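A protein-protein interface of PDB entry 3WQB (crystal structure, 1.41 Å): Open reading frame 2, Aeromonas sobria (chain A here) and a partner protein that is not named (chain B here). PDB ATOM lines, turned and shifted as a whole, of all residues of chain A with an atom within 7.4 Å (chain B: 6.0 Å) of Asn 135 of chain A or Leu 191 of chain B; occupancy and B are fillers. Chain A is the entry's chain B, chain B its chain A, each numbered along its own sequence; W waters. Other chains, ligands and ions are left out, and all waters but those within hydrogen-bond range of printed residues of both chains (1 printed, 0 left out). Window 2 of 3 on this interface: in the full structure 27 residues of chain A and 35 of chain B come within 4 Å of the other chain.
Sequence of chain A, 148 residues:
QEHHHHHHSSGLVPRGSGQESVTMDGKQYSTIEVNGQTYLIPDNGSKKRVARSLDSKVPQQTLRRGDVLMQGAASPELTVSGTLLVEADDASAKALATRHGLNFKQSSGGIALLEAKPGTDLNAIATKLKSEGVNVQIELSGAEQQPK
N of Glu 87 of chain A lies within hydrogen-bond range of O of Asn 135 of chain A (3.0 Å). NE2 of Gln 155 of chain B lies within hydrogen-bond range of O of Asp 192 of chain B (3.1 Å). OE1 of Gln 195 of chain B sits at hydrogen-bond distance from NE2 of Gln 155 of chain B, 2.9 Å away. The side-chain amino group (NZ) of Lys 130 of chain A sits at hydrogen-bond distance from the backbone carbonyl oxygen (O) of Val 136 of chain A (3.3 Å). The side-chain amide nitrogen of Gln 193 of chain B sits at hydrogen-bond distance from the side-chain hydroxyl of Ser 190 of chain B (2.8 Å). The side-chain hydroxyl (OG) of Ser 190 of chain B lies within hydrogen-bond range of the side-chain carboxylate (OD1) of Asp 192 of chain B (2.6 Å).
Water W1 bridges OG of Ser 108 of chain A (2.8 Å) and O of Gln 195 of chain B (2.8 Å).
Among the printed residues, merely in contact across the chains: Leu 85 of chain A with Leu 191 of chain B (3.5 Å), Leu 85 of chain A with Asp 192 of chain B (3.5 Å), Glu 87 of chain A with Leu 191 of chain B (3.8 Å), Ile 111 of chain A with Leu 191 of chain B (3.6 Å), Asn 135 of chain A with Leu 191 of chain B (3.6 Å), Val 136 of chain A with Leu 191 of chain B (3.97 Å) and Gln 137 of chain A with Ser 190 of chain B (3.7 Å).
Hydrophobic or aromatic side chains of chain B within 4 Å of the printed part of chain A: Leu 191. Of the 20 printed residues of chain A, 7 touch a printed residue of chain B. Hydrophobic or aromatic side chains of chain A that line the printed part of chain B: Leu 85 and Ile 111. Among the printed residues, no Asp or Glu carboxylate lies within 4 Å of a Lys or Arg side-chain nitrogen of the other chain.
Ala 112 of chain A touches none of the printed residues of chain B. Leu 129 of chain A touches none of the printed residues of chain B. Asn 135 of chain A touches one residue of chain B. Printed residues of chain B within 4 Å of Val 136 of chain A: Leu 191. Printed residues of chain A within 4 Å of Gln 195 of chain B: Ser 108 (3.0 Å) and Ile 111 (2.9 Å). The nearest printed residue of chain B that does not touch Asn 135 of chain A is Asn 189 of chain B (6.3 Å). The nearest residue of chain A that does not touch Leu 191 of chain B is Val 86 of chain A (4.3 Å).
The backbone NH of Leu 191 of chain B is in hydrogen-bond range of the side-chain amide oxygen of Gln 137 of chain A (3.4 Å). NE2 of Gln 195 of chain B is in hydrogen-bond range of O of Ser 108 of chain A, 3.0 Å away. The side-chain amide nitrogen (NE2) of Gln 195 of chain B is in hydrogen-bond range of the backbone carbonyl oxygen (O) of Ile 111 of chain A (2.9 Å). The side-chain amide oxygen (OE1) of Gln 137 of chain A lies within hydrogen-bond range of the backbone NH (N) of Asp 192 of chain B (2.8 Å).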
ATOM      1  N   LEU A  84     -24.561  18.890 -24.462  1.00  0.00           N
ATOM      2  CA  LEU A  84     -25.588  19.894 -24.220  1.00  0.00           C
ATOM      3  C   LEU A  84     -25.102  20.836 -23.134  1.00  0.00           C
ATOM      4  O   LEU A  84     -24.600  20.389 -22.096  1.00  0.00           O
ATOM      5  CB  LEU A  84     -26.890  19.231 -23.748  1.00  0.00           C
ATOM      6  CG  LEU A  84     -27.581  18.223 -24.664  1.00  0.00           C
ATOM      7  CD1 LEU A  84     -28.363  17.221 -23.836  1.00  0.00           C
ATOM      8  CD2 LEU A  84     -28.495  18.919 -25.637  1.00  0.00           C
ATOM      9  N   LEU A  85     -25.240  22.135 -23.375  1.00  0.00           N
ATOM     10  CA  LEU A  85     -25.006  23.142 -22.334  1.00  0.00           C
ATOM     11  C   LEU A  85     -26.342  23.458 -21.692  1.00  0.00           C
ATOM     12  O   LEU A  85     -27.326  23.705 -22.386  1.00  0.00           O
ATOM     13  CB  LEU A  85     -24.394  24.423 -22.907  1.00  0.00           C
ATOM     14  CG  LEU A  85     -23.101  24.367 -23.726  1.00  0.00           C
ATOM     15  CD1 LEU A  85     -22.525  25.766 -23.809  1.00  0.00           C
ATOM     16  CD2 LEU A  85     -22.059  23.409 -23.182  1.00  0.00           C
ATOM     17  N   VAL A  86     -26.371  23.432 -20.365  1.00  0.00           N
ATOM     18  CA  VAL A  86     -27.593  23.660 -19.601  1.00  0.00           C
ATOM     19  C   VAL A  86     -27.316  24.699 -18.517  1.00  0.00           C
ATOM     20  O   VAL A  86     -26.349  24.570 -17.763  1.00  0.00           O
ATOM     21  CB  VAL A  86     -28.098  22.331 -18.965  1.00  0.00           C
ATOM     22  CG1 VAL A  86     -29.193  22.575 -17.941  1.00  0.00           C
ATOM     23  CG2 VAL A  86     -28.601  21.390 -20.040  1.00  0.00           C
ATOM     24  N   GLU A  87     -28.153  25.733 -18.447  1.00  0.00           N
ATOM     25  CA  GLU A  87     -28.027  26.722 -17.379  1.00  0.00           C
ATOM     26  C   GLU A  87     -28.739  26.236 -16.117  1.00  0.00           C
ATOM     27  O   GLU A  87     -29.959  26.354 -15.984  1.00  0.00           O
ATOM     28  CB  GLU A  87     -28.532  28.098 -17.814  1.00  0.00           C
ATOM     29  CG  GLU A  87     -28.143  29.203 -16.837  1.00  0.00           C
ATOM     30  CD  GLU A  87     -28.280  30.596 -17.414  1.00  0.00           C
ATOM     31  OE1 GLU A  87     -29.074  30.787 -18.361  1.00  0.00           O
ATOM     32  OE2 GLU A  87     -27.589  31.506 -16.906  1.00  0.00           O
ATOM     33  N   ALA A  88     -27.954  25.666 -15.213  1.00  0.00           N
ATOM     34  CA  ALA A  88     -28.447  25.136 -13.948  1.00  0.00           C
ATOM     35  C   ALA A  88     -27.257  24.994 -13.017  1.00  0.00           C
ATOM     36  O   ALA A  88     -26.126  24.804 -13.472  1.00  0.00           O
ATOM     37  CB  ALA A  88     -29.105  23.780 -14.162  1.00  0.00           C
ATOM     38  N   LEU A  96     -31.030  16.641 -13.407  1.00  0.00           N
ATOM     39  CA  LEU A  96     -31.515  16.722 -14.787  1.00  0.00           C
ATOM     40  C   LEU A  96     -30.843  15.706 -15.709  1.00  0.00           C
ATOM     41  O   LEU A  96     -31.469  15.208 -16.643  1.00  0.00           O
ATOM     42  CB  LEU A  96     -31.330  18.138 -15.346  1.00  0.00           C
ATOM     43  CG  LEU A  96     -32.516  19.112 -15.387  1.00  0.00           C
ATOM     44  CD1 LEU A  96     -33.208  19.285 -14.032  1.00  0.00           C
ATOM     45  CD2 LEU A  96     -32.052  20.459 -15.927  1.00  0.00           C
ATOM     46  N   SER A 108     -19.146  25.285 -15.430  1.00  0.00           N
ATOM     47  CA  SER A 108     -18.438  26.542 -15.251  1.00  0.00           C
ATOM     48  C   SER A 108     -19.440  27.676 -15.397  1.00  0.00           C
ATOM     49  O   SER A 108     -20.265  27.657 -16.312  1.00  0.00           O
ATOM     50  CB  SER A 108     -17.358  26.679 -16.322  1.00  0.00           C
ATOM     51  OG  SER A 108     -16.546  27.810 -16.085  1.00  0.00           O
ATOM     52  N   GLY A 110     -22.103  28.556 -13.823  1.00  0.00           N
ATOM     53  CA  GLY A 110     -23.517  28.197 -13.709  1.00  0.00           C
ATOM     54  C   GLY A 110     -24.070  27.486 -14.934  1.00  0.00           C
ATOM     55  O   GLY A 110     -25.284  27.329 -15.085  1.00  0.00           O
ATOM     56  N   ILE A 111     -23.175  27.057 -15.814  1.00  0.00           N
ATOM     57  CA  ILE A 111     -23.572  26.342 -17.018  1.00  0.00           C
ATOM     58  C   ILE A 111     -22.893  24.975 -17.064  1.00  0.00           C
ATOM     59  O   ILE A 111     -21.669  24.870 -17.018  1.00  0.00           O
ATOM     60  CB  ILE A 111     -23.296  27.191 -18.284  1.00  0.00           C
ATOM     61  CG1 ILE A 111     -24.210  28.428 -18.285  1.00  0.00           C
ATOM     62  CG2 ILE A 111     -23.474  26.349 -19.559  1.00  0.00           C
ATOM     63  CD1 ILE A 111     -23.745  29.551 -19.203  1.00  0.00           C
ATOM     64  N   ALA A 112     -23.709  23.927 -17.114  1.00  0.00           N
ATOM     65  CA  ALA A 112     -23.211  22.570 -17.098  1.00  0.00           C
ATOM     66  C   ALA A 112     -23.101  21.997 -18.504  1.00  0.00           C
ATOM     67  O   ALA A 112     -23.905  22.320 -19.379  1.00  0.00           O
ATOM     68  CB  ALA A 112     -24.112  21.691 -16.243  1.00  0.00           C
ATOM     69  N   ALA A 126     -33.583  18.431 -25.828  1.00  0.00           N
ATOM     70  CA  ALA A 126     -33.556  19.893 -25.740  1.00  0.00           C
ATOM     71  C   ALA A 126     -34.956  20.499 -25.689  1.00  0.00           C
ATOM     72  O   ALA A 126     -35.211  21.403 -24.891  1.00  0.00           O
ATOM     73  CB  ALA A 126     -32.756  20.488 -26.894  1.00  0.00           C
ATOM     74  N   LEU A 129     -36.412  19.851 -22.215  1.00  0.00           N
ATOM     75  CA  LEU A 129     -35.801  20.753 -21.238  1.00  0.00           C
ATOM     76  C   LEU A 129     -36.337  22.180 -21.342  1.00  0.00           C
ATOM     77  O   LEU A 129     -36.555  22.833 -20.319  1.00  0.00           O
ATOM     78  CB  LEU A 129     -34.273  20.736 -21.360  1.00  0.00           C
ATOM     79  CG  LEU A 129     -33.543  19.524 -20.772  1.00  0.00           C
ATOM     80  CD1 LEU A 129     -32.118  19.454 -21.303  1.00  0.00           C
ATOM     81  CD2 LEU A 129     -33.549  19.535 -19.242  1.00  0.00           C
ATOM     82  N   LYS A 130     -36.549  22.651 -22.570  1.00  0.00           N
ATOM     83  CA  LYS A 130     -37.154  23.964 -22.815  1.00  0.00           C
ATOM     84  C   LYS A 130     -38.548  24.048 -22.196  1.00  0.00           C
ATOM     85  O   LYS A 130     -38.881  25.035 -21.535  1.00  0.00           O
ATOM     86  CB  LYS A 130     -37.229  24.269 -24.317  1.00  0.00           C
ATOM     87  CG  LYS A 130     -35.892  24.593 -24.982  1.00  0.00           C
ATOM     88  CD  LYS A 130     -35.295  25.895 -24.461  1.00  0.00           C
ATOM     89  CE  LYS A 130     -34.058  26.293 -25.251  1.00  0.00           C
ATOM     90  NZ  LYS A 130     -33.183  27.203 -24.457  1.00  0.00           N
ATOM     91  N   GLU A 132     -39.633  22.394 -19.745  1.00  0.00           N
ATOM     92  CA  GLU A 132     -39.454  22.371 -18.294  1.00  0.00           C
ATOM     93  C   GLU A 132     -38.888  23.691 -17.751  1.00  0.00           C
ATOM     94  O   GLU A 132     -38.664  23.827 -16.543  1.00  0.00           O
ATOM     95  CB  GLU A 132     -38.553  21.197 -17.882  1.00  0.00           C
ATOM     96  CG  GLU A 132     -39.183  19.815 -18.079  1.00  0.00           C
ATOM     97  CD  GLU A 132     -38.257  18.656 -17.705  1.00  0.00           C
ATOM     98  OE1 GLU A 132     -38.666  17.491 -17.908  1.00  0.00           O
ATOM     99  OE2 GLU A 132     -37.129  18.896 -17.215  1.00  0.00           O
ATOM    100  N   GLY A 133     -38.661  24.654 -18.643  1.00  0.00           N
ATOM    101  CA  GLY A 133     -38.173  25.984 -18.262  1.00  0.00           C
ATOM    102  C   GLY A 133     -36.666  26.089 -18.100  1.00  0.00           C
ATOM    103  O   GLY A 133     -36.165  26.999 -17.434  1.00  0.00           O
ATOM    104  N   VAL A 134     -35.940  25.159 -18.711  1.00  0.00           N
ATOM    105  CA  VAL A 134     -34.485  25.133 -18.619  1.00  0.00           C
ATOM    106  C   VAL A 134     -33.880  25.668 -19.916  1.00  0.00           C
ATOM    107  O   VAL A 134     -34.281  25.259 -21.006  1.00  0.00           O
ATOM    108  CB  VAL A 134     -33.964  23.703 -18.327  1.00  0.00           C
ATOM    109  CG1 VAL A 134     -32.465  23.713 -18.076  1.00  0.00           C
ATOM    110  CG2 VAL A 134     -34.700  23.094 -17.133  1.00  0.00           C
ATOM    111  N   ASN A 135     -32.945  26.607 -19.787  1.00  0.00           N
ATOM    112  CA  ASN A 135     -32.171  27.099 -20.926  1.00  0.00           C
ATOM    113  C   ASN A 135     -31.127  26.069 -21.344  1.00  0.00           C
ATOM    114  O   ASN A 135     -30.299  25.650 -20.540  1.00  0.00           O
ATOM    115  CB  ASN A 135     -31.499  28.436 -20.595  1.00  0.00           C
ATOM    116  CG  ASN A 135     -32.400  29.632 -20.860  1.00  0.00           C
ATOM    117  OD1 ASN A 135     -33.584  29.627 -20.522  1.00  0.00           O
ATOM    118  ND2 ASN A 135     -31.833  30.668 -21.471  1.00  0.00           N
ATOM    119  N   VAL A 136     -31.196  25.652 -22.601  1.00  0.00           N
ATOM    120  CA  VAL A 136     -30.338  24.588 -23.122  1.00  0.00           C
ATOM    121  C   VAL A 136     -29.781  24.966 -24.498  1.00  0.00           C
ATOM    122  O   VAL A 136     -30.455  25.616 -25.291  1.00  0.00           O
ATOM    123  CB  VAL A 136     -31.105  23.227 -23.177  1.00  0.00           C
ATOM    124  CG1 VAL A 136     -32.393  23.340 -23.998  1.00  0.00           C
ATOM    125  CG2 VAL A 136     -30.225  22.101 -23.716  1.00  0.00           C
ATOM    126  N   GLN A 137     -28.544  24.556 -24.766  1.00  0.00           N
ATOM    127  CA  GLN A 137     -27.937  24.733 -26.077  1.00  0.00           C
ATOM    128  C   GLN A 137     -27.274  23.427 -26.498  1.00  0.00           C
ATOM    129  O   GLN A 137     -26.457  22.866 -25.761  1.00  0.00           O
ATOM    130  CB  GLN A 137     -26.912  25.881 -26.063  1.00  0.00           C
ATOM    131  CG  GLN A 137     -26.259  26.186 -27.423  1.00  0.00           C
ATOM    132  CD  GLN A 137     -25.134  27.209 -27.324  1.00  0.00           C
ATOM    133  OE1 GLN A 137     -24.537  27.385 -26.269  1.00  0.00           O
ATOM    134  NE2 GLN A 137     -24.850  27.894 -28.426  1.00  0.00           N
ATOM    135  N   ILE A 138     -27.657  22.930 -27.668  1.00  0.00           N
ATOM    136  CA  ILE A 138     -26.991  21.780 -28.271  1.00  0.00           C
ATOM    137  C   ILE A 138     -25.681  22.264 -28.882  1.00  0.00           C
ATOM    138  O   ILE A 138     -25.683  23.170 -29.721  1.00  0.00           O
ATOM    139  CB  ILE A 138     -27.869  21.132 -29.369  1.00  0.00           C
ATOM    140  CG1 ILE A 138     -29.190  20.646 -28.763  1.00  0.00           C
ATOM    141  CG2 ILE A 138     -27.125  19.979 -30.042  1.00  0.00           C
ATOM    142  CD1 ILE A 138     -30.276  20.311 -29.772  1.00  0.00           C
ATOM    143  N   GLN B 155     -16.339  23.280 -26.613  1.00  0.00           N
ATOM    144  CA  GLN B 155     -16.498  24.096 -25.412  1.00  0.00           C
ATOM    145  C   GLN B 155     -15.576  23.651 -24.272  1.00  0.00           C
ATOM    146  O   GLN B 155     -14.958  24.487 -23.614  1.00  0.00           O
ATOM    147  CB  GLN B 155     -17.957  24.114 -24.942  1.00  0.00           C
ATOM    148  CG  GLN B 155     -18.244  25.182 -23.866  1.00  0.00           C
ATOM    149  CD  GLN B 155     -18.273  26.594 -24.411  1.00  0.00           C
ATOM    150  OE1 GLN B 155     -18.133  26.806 -25.613  1.00  0.00           O
ATOM    151  NE2 GLN B 155     -18.492  27.572 -23.532  1.00  0.00           N
ATOM    152  N   ASN B 189     -25.776  36.238 -26.608  1.00  0.00           N
ATOM    153  CA  ASN B 189     -26.402  35.651 -25.422  1.00  0.00           C
ATOM    154  C   ASN B 189     -26.505  34.128 -25.367  1.00  0.00           C
ATOM    155  O   ASN B 189     -27.067  33.587 -24.410  1.00  0.00           O
ATOM    156  CB  ASN B 189     -27.781  36.280 -25.208  1.00  0.00           C
ATOM    157  CG  ASN B 189     -27.697  37.746 -24.856  1.00  0.00           C
ATOM    158  OD1 ASN B 189     -26.925  38.144 -23.975  1.00  0.00           O
ATOM    159  ND2 ASN B 189     -28.494  38.561 -25.537  1.00  0.00           N
ATOM    160  N   SER B 190     -25.962  33.438 -26.365  1.00  0.00           N
ATOM    161  CA  SER B 190     -25.953  31.978 -26.363  1.00  0.00           C
ATOM    162  C   SER B 190     -25.196  31.466 -25.136  1.00  0.00           C
ATOM    163  O   SER B 190     -24.324  32.151 -24.601  1.00  0.00           O
ATOM    164  CB  SER B 190     -25.338  31.432 -27.651  1.00  0.00           C
ATOM    165  OG  SER B 190     -23.968  31.770 -27.739  1.00  0.00           O
ATOM    166  N   LEU B 191     -25.532  30.263 -24.688  1.00  0.00           N
ATOM    167  CA  LEU B 191     -24.924  29.726 -23.475  1.00  0.00           C
ATOM    168  C   LEU B 191     -23.413  29.544 -23.576  1.00  0.00           C
ATOM    169  O   LEU B 191     -22.700  29.785 -22.602  1.00  0.00           O
ATOM    170  CB  LEU B 191     -25.596  28.419 -23.081  1.00  0.00           C
ATOM    171  CG  LEU B 191     -27.014  28.534 -22.507  1.00  0.00           C
ATOM    172  CD1 LEU B 191     -27.483  27.159 -22.113  1.00  0.00           C
ATOM    173  CD2 LEU B 191     -27.075  29.476 -21.308  1.00  0.00           C
ATOM    174  N   ASP B 192     -22.918  29.156 -24.748  1.00  0.00           N
ATOM    175  CA  ASP B 192     -21.480  28.975 -24.922  1.00  0.00           C
ATOM    176  C   ASP B 192     -20.750  30.298 -24.695  1.00  0.00           C
ATOM    177  O   ASP B 192     -19.698  30.326 -24.062  1.00  0.00           O
ATOM    178  CB  ASP B 192     -21.131  28.351 -26.292  1.00  0.00           C
ATOM    179  CG  ASP B 192     -21.301  29.315 -27.446  1.00  0.00           C
ATOM    180  OD1 ASP B 192     -22.451  29.688 -27.745  1.00  0.00           O
ATOM    181  OD2 ASP B 192     -20.276  29.706 -28.048  1.00  0.00           O
ATOM    182  N   GLN B 193     -21.314  31.384 -25.218  1.00  0.00           N
ATOM    183  CA  GLN B 193     -20.708  32.708 -25.085  1.00  0.00           C
ATOM    184  C   GLN B 193     -20.856  33.264 -23.676  1.00  0.00           C
ATOM    185  O   GLN B 193     -19.922  33.864 -23.151  1.00  0.00           O
ATOM    186  CB  GLN B 193     -21.303  33.680 -26.097  1.00  0.00           C
ATOM    187  CG  GLN B 193     -21.090  33.258 -27.537  1.00  0.00           C
ATOM    188  CD  GLN B 193     -21.675  34.245 -28.507  1.00  0.00           C
ATOM    189  OE1 GLN B 193     -21.063  35.266 -28.795  1.00  0.00           O
ATOM    190  NE2 GLN B 193     -22.871  33.957 -29.010  1.00  0.00           N
ATOM    191  N   SER B 194     -22.026  33.065 -23.078  1.00  0.00           N
ATOM    192  CA  SER B 194     -22.255  33.483 -21.697  1.00  0.00           C
ATOM    193  C   SER B 194     -21.269  32.801 -20.750  1.00  0.00           C
ATOM    194  O   SER B 194     -20.691  33.444 -19.878  1.00  0.00           O
ATOM    195  CB  SER B 194     -23.698  33.190 -21.272  1.00  0.00           C
ATOM    196  OG  SER B 194     -23.925  33.549 -19.923  1.00  0.00           O
ATOM    197  N   GLN B 195     -21.048  31.506 -20.957  1.00  0.00           N
ATOM    198  CA  GLN B 195     -20.142  30.743 -20.108  1.00  0.00           C
ATOM    199  C   GLN B 195     -18.719  31.286 -20.204  1.00  0.00           C
ATOM    200  O   GLN B 195     -18.038  31.443 -19.184  1.00  0.00           O
ATOM    201  CB  GLN B 195     -20.183  29.261 -20.466  1.00  0.00           C
ATOM    202  CG  GLN B 195     -19.334  28.386 -19.558  1.00  0.00           C
ATOM    203  CD  GLN B 195     -19.487  26.918 -19.861  1.00  0.00           C
ATOM    204  OE1 GLN B 195     -19.257  26.486 -20.985  1.00  0.00           O
ATOM    205  NE2 GLN B 195     -19.861  26.131 -18.852  1.00  0.00           N
ATOM    206  N   LEU B 196     -18.263  31.581 -21.418  1.00  0.00           N
ATOM    207  CA  LEU B 196     -16.917  32.130 -21.574  1.00  0.00           C
ATOM    208  C   LEU B 196     -16.824  33.568 -21.045  1.00  0.00           C
ATOM    209  O   LEU B 196     -15.838  33.931 -20.406  1.00  0.00           O
ATOM    210  CB  LEU B 196     -16.428  32.011 -23.022  1.00  0.00           C
ATOM    211  CG  LEU B 196     -16.129  30.568 -23.438  1.00  0.00           C
ATOM    212  CD1 LEU B 196     -15.935  30.462 -24.940  1.00  0.00           C
ATOM    213  CD2 LEU B 196     -14.910  30.010 -22.707  1.00  0.00           C
HETATM  214  O   HOH W   1     -17.741  30.287 -16.627  1.00  0.00           O
